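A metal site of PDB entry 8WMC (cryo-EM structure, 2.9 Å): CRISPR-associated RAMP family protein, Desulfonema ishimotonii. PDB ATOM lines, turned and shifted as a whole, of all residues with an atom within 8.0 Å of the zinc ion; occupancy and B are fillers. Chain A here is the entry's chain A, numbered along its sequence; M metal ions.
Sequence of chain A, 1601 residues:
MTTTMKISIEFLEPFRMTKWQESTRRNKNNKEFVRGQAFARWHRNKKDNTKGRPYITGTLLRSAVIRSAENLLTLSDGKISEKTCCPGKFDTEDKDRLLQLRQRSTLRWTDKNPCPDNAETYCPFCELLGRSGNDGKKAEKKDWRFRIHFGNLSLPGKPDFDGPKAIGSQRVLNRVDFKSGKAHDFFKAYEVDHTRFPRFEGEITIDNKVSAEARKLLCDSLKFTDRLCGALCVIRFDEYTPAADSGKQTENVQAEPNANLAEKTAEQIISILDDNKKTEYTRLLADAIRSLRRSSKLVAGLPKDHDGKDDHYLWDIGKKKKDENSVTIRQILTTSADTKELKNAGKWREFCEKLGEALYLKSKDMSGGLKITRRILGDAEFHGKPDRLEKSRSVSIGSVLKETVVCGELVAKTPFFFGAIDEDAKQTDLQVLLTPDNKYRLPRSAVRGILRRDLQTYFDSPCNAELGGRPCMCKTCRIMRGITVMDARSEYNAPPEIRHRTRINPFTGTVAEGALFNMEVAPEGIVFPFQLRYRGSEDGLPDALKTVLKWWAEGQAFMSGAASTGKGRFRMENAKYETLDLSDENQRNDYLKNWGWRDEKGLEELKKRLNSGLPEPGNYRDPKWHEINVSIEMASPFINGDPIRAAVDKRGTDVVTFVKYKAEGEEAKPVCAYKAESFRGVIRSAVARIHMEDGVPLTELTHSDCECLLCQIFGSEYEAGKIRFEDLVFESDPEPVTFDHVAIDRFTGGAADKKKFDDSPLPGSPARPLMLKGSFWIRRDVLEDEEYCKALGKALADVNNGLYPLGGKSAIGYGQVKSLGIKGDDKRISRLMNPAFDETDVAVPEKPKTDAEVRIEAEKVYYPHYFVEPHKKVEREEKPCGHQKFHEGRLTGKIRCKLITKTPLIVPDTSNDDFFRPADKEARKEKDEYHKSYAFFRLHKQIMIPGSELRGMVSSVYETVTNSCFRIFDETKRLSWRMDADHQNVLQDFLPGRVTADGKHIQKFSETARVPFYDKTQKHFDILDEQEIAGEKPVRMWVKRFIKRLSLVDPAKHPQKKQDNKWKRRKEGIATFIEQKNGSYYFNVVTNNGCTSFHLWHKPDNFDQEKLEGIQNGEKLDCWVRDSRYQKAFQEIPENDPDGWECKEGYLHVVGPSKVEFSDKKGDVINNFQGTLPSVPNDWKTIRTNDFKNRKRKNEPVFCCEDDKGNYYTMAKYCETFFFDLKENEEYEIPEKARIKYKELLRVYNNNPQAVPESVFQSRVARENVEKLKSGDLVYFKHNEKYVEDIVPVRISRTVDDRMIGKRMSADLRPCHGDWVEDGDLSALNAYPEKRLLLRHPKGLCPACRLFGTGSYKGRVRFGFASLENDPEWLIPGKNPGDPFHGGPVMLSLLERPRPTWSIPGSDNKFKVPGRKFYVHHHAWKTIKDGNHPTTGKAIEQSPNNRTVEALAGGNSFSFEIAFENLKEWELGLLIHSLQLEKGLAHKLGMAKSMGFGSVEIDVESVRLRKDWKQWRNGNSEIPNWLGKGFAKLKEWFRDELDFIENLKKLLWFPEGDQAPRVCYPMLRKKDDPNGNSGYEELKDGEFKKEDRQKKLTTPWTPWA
NE2 of His 703 is in hydrogen-bond range of O of Leu 698 (2.8 Å).
SG of Cys 708 sits close to N of Leu 710 (3.4 Å).
ND1 of His 703 binds the zinc ion (2.1 Å).
The zinc ion is bound by SG of Cys 708 (2.3 Å).
The side-chain sulfur (SG) of Cys 706 binds the zinc ion (2.3 Å).
SG of Cys 711 is bound to the zinc ion (2.3 Å).
Within 4 Å of the zinc ion: His 703, Cys 706, Cys 708 and Cys 711.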
ATOM      1  N   ARG A 684      21.545   8.672  -0.866  1.00  0.00           N
ATOM      2  CA  ARG A 684      20.479   9.405  -0.180  1.00  0.00           C
ATOM      3  C   ARG A 684      19.256   8.524   0.033  1.00  0.00           C
ATOM      4  O   ARG A 684      18.633   8.562   1.104  1.00  0.00           O
ATOM      5  CB  ARG A 684      20.116  10.657  -0.965  1.00  0.00           C
ATOM      6  CG  ARG A 684      18.761  11.254  -0.628  1.00  0.00           C
ATOM      7  CD  ARG A 684      18.658  12.700  -1.068  1.00  0.00           C
ATOM      8  NE  ARG A 684      17.302  13.007  -1.518  1.00  0.00           N
ATOM      9  CZ  ARG A 684      16.724  14.206  -1.437  1.00  0.00           C
ATOM     10  NH1 ARG A 684      17.345  15.258  -0.941  1.00  0.00           N
ATOM     11  NH2 ARG A 684      15.466  14.337  -1.876  1.00  0.00           N
ATOM     12  N   GLU A 693      10.564   9.971  10.961  1.00  0.00           N
ATOM     13  CA  GLU A 693      10.283  11.188  11.713  1.00  0.00           C
ATOM     14  C   GLU A 693       8.851  11.106  12.215  1.00  0.00           C
ATOM     15  O   GLU A 693       7.919  10.986  11.409  1.00  0.00           O
ATOM     16  CB  GLU A 693      10.487  12.424  10.841  1.00  0.00           C
ATOM     17  CG  GLU A 693      10.491  13.737  11.628  1.00  0.00           C
ATOM     18  CD  GLU A 693      10.479  14.959  10.729  1.00  0.00           C
ATOM     19  OE1 GLU A 693       9.668  14.986   9.781  1.00  0.00           O
ATOM     20  OE2 GLU A 693      11.279  15.885  10.967  1.00  0.00           O
ATOM     21  N   LEU A 698      11.146   9.169   6.188  1.00  0.00           N
ATOM     22  CA  LEU A 698      11.628  10.394   5.553  1.00  0.00           C
ATOM     23  C   LEU A 698      11.402  10.410   4.046  1.00  0.00           C
ATOM     24  O   LEU A 698      11.417  11.486   3.444  1.00  0.00           O
ATOM     25  CB  LEU A 698      13.115  10.593   5.845  1.00  0.00           C
ATOM     26  CG  LEU A 698      13.524  10.633   7.322  1.00  0.00           C
ATOM     27  CD1 LEU A 698      15.037  10.679   7.447  1.00  0.00           C
ATOM     28  CD2 LEU A 698      12.895  11.811   8.031  1.00  0.00           C
ATOM     29  N   LEU A 701       7.985  12.480   3.172  1.00  0.00           N
ATOM     30  CA  LEU A 701       7.815  13.900   3.444  1.00  0.00           C
ATOM     31  C   LEU A 701       8.070  14.721   2.184  1.00  0.00           C
ATOM     32  O   LEU A 701       8.746  14.295   1.255  1.00  0.00           O
ATOM     33  CB  LEU A 701       8.751  14.354   4.563  1.00  0.00           C
ATOM     34  CG  LEU A 701       8.746  13.518   5.844  1.00  0.00           C
ATOM     35  CD1 LEU A 701       9.736  14.090   6.846  1.00  0.00           C
ATOM     36  CD2 LEU A 701       7.351  13.455   6.442  1.00  0.00           C
ATOM     37  N   THR A 702       7.499  15.930   2.178  1.00  0.00           N
ATOM     38  CA  THR A 702       7.683  16.831   1.045  1.00  0.00           C
ATOM     39  C   THR A 702       9.073  17.454   1.022  1.00  0.00           C
ATOM     40  O   THR A 702       9.601  17.752  -0.055  1.00  0.00           O
ATOM     41  CB  THR A 702       6.611  17.920   1.080  1.00  0.00           C
ATOM     42  OG1 THR A 702       5.309  17.331   1.017  1.00  0.00           O
ATOM     43  CG2 THR A 702       6.789  18.881  -0.092  1.00  0.00           C
ATOM     44  N   HIS A 703       9.671  17.660   2.197  1.00  0.00           N
ATOM     45  CA  HIS A 703      11.002  18.238   2.375  1.00  0.00           C
ATOM     46  C   HIS A 703      11.105  19.682   1.892  1.00  0.00           C
ATOM     47  O   HIS A 703      12.217  20.207   1.766  1.00  0.00           O
ATOM     48  CB  HIS A 703      12.082  17.391   1.697  1.00  0.00           C
ATOM     49  CG  HIS A 703      12.303  16.065   2.349  1.00  0.00           C
ATOM     50  ND1 HIS A 703      12.615  15.928   3.685  1.00  0.00           N
ATOM     51  CD2 HIS A 703      12.254  14.806   1.834  1.00  0.00           C
ATOM     52  CE1 HIS A 703      12.748  14.641   3.967  1.00  0.00           C
ATOM     53  NE2 HIS A 703      12.540  13.947   2.869  1.00  0.00           N
ATOM     54  N   SER A 704       9.985  20.347   1.627  1.00  0.00           N
ATOM     55  CA  SER A 704       9.972  21.778   1.319  1.00  0.00           C
ATOM     56  C   SER A 704       9.791  22.551   2.615  1.00  0.00           C
ATOM     57  O   SER A 704       8.762  22.429   3.272  1.00  0.00           O
ATOM     58  CB  SER A 704       8.859  22.109   0.323  1.00  0.00           C
ATOM     59  OG  SER A 704       8.990  21.350  -0.862  1.00  0.00           O
ATOM     60  N   ASP A 705      10.799  23.344   2.983  1.00  0.00           N
ATOM     61  CA  ASP A 705      10.826  24.039   4.265  1.00  0.00           C
ATOM     62  C   ASP A 705      10.782  23.030   5.411  1.00  0.00           C
ATOM     63  O   ASP A 705       9.878  23.022   6.245  1.00  0.00           O
ATOM     64  CB  ASP A 705       9.677  25.048   4.360  1.00  0.00           C
ATOM     65  CG  ASP A 705       9.905  26.092   5.431  1.00  0.00           C
ATOM     66  OD1 ASP A 705      10.801  26.932   5.255  1.00  0.00           O
ATOM     67  OD2 ASP A 705       9.178  26.071   6.452  1.00  0.00           O
ATOM     68  N   CYS A 706      11.800  22.159   5.437  1.00  0.00           N
ATOM     69  CA  CYS A 706      11.891  21.053   6.362  1.00  0.00           C
ATOM     70  C   CYS A 706      13.234  21.095   7.087  1.00  0.00           C
ATOM     71  O   CYS A 706      14.200  21.684   6.598  1.00  0.00           O
ATOM     72  CB  CYS A 706      11.719  19.711   5.636  1.00  0.00           C
ATOM     73  SG  CYS A 706      11.956  18.246   6.665  1.00  0.00           S
ATOM     74  N   GLU A 707      13.274  20.458   8.257  1.00  0.00           N
ATOM     75  CA  GLU A 707      14.471  20.433   9.098  1.00  0.00           C
ATOM     76  C   GLU A 707      14.697  19.030   9.651  1.00  0.00           C
ATOM     77  O   GLU A 707      15.016  18.857  10.833  1.00  0.00           O
ATOM     78  CB  GLU A 707      14.365  21.443  10.241  1.00  0.00           C
ATOM     79  CG  GLU A 707      14.044  22.874   9.819  1.00  0.00           C
ATOM     80  CD  GLU A 707      13.785  23.794  10.995  1.00  0.00           C
ATOM     81  OE1 GLU A 707      12.601  24.050  11.303  1.00  0.00           O
ATOM     82  OE2 GLU A 707      14.767  24.247  11.615  1.00  0.00           O
ATOM     83  N   CYS A 708      14.529  18.019   8.811  1.00  0.00           N
ATOM     84  CA  CYS A 708      14.741  16.633   9.210  1.00  0.00           C
ATOM     85  C   CYS A 708      16.219  16.277   9.098  1.00  0.00           C
ATOM     86  O   CYS A 708      17.047  17.069   8.658  1.00  0.00           O
ATOM     87  CB  CYS A 708      13.887  15.690   8.361  1.00  0.00           C
ATOM     88  SG  CYS A 708      14.507  15.450   6.688  1.00  0.00           S
ATOM     89  N   LEU A 709      16.556  15.041   9.499  1.00  0.00           N
ATOM     90  CA  LEU A 709      17.936  14.590   9.420  1.00  0.00           C
ATOM     91  C   LEU A 709      18.433  14.563   7.986  1.00  0.00           C
ATOM     92  O   LEU A 709      19.568  14.982   7.698  1.00  0.00           O
ATOM     93  CB  LEU A 709      18.052  13.199  10.054  1.00  0.00           C
ATOM     94  CG  LEU A 709      19.435  12.557  10.089  1.00  0.00           C
ATOM     95  CD1 LEU A 709      19.719  11.956  11.450  1.00  0.00           C
ATOM     96  CD2 LEU A 709      19.557  11.498   9.005  1.00  0.00           C
ATOM     97  N   LEU A 710      17.602  14.089   7.063  1.00  0.00           N
ATOM     98  CA  LEU A 710      17.986  14.058   5.655  1.00  0.00           C
ATOM     99  C   LEU A 710      18.246  15.467   5.128  1.00  0.00           C
ATOM    100  O   LEU A 710      19.226  15.687   4.403  1.00  0.00           O
ATOM    101  CB  LEU A 710      16.905  13.373   4.823  1.00  0.00           C
ATOM    102  CG  LEU A 710      17.328  12.852   3.450  1.00  0.00           C
ATOM    103  CD1 LEU A 710      18.119  11.564   3.589  1.00  0.00           C
ATOM    104  CD2 LEU A 710      16.122  12.657   2.564  1.00  0.00           C
ATOM    105  N   CYS A 711      17.385  16.420   5.469  1.00  0.00           N
ATOM    106  CA  CYS A 711      17.572  17.791   5.010  1.00  0.00           C
ATOM    107  C   CYS A 711      18.841  18.400   5.596  1.00  0.00           C
ATOM    108  O   CYS A 711      19.618  19.034   4.891  1.00  0.00           O
ATOM    109  CB  CYS A 711      16.351  18.636   5.358  1.00  0.00           C
ATOM    110  SG  CYS A 711      14.924  18.336   4.288  1.00  0.00           S
ATOM    111  N   GLN A 712      19.078  18.176   6.896  1.00  0.00           N
ATOM    112  CA  GLN A 712      20.282  18.715   7.517  1.00  0.00           C
ATOM    113  C   GLN A 712      21.551  18.133   6.918  1.00  0.00           C
ATOM    114  O   GLN A 712      22.556  18.844   6.791  1.00  0.00           O
ATOM    115  CB  GLN A 712      20.259  18.487   9.031  1.00  0.00           C
ATOM    116  CG  GLN A 712      19.175  19.260   9.761  1.00  0.00           C
ATOM    117  CD  GLN A 712      19.170  18.980  11.252  1.00  0.00           C
ATOM    118  OE1 GLN A 712      19.942  18.154  11.744  1.00  0.00           O
ATOM    119  NE2 GLN A 712      18.299  19.668  11.979  1.00  0.00           N
ATOM    120  N   GLY A 715      21.219  18.822   2.499  1.00  0.00           N
ATOM    121  CA  GLY A 715      20.792  20.117   1.996  1.00  0.00           C
ATOM    122  C   GLY A 715      19.358  20.099   1.495  1.00  0.00           C
ATOM    123  O   GLY A 715      18.716  19.054   1.345  1.00  0.00           O
ATOM    124  N   SER A 716      18.838  21.295   1.225  1.00  0.00           N
ATOM    125  CA  SER A 716      17.475  21.474   0.755  1.00  0.00           C
ATOM    126  C   SER A 716      17.424  22.740  -0.097  1.00  0.00           C
ATOM    127  O   SER A 716      18.467  23.315  -0.449  1.00  0.00           O
ATOM    128  CB  SER A 716      16.496  21.526   1.931  1.00  0.00           C
ATOM    129  OG  SER A 716      16.787  22.618   2.792  1.00  0.00           O
HETATM  130 ZN    ZN M   1      13.380  16.968   5.356  1.00  0.00          ZN
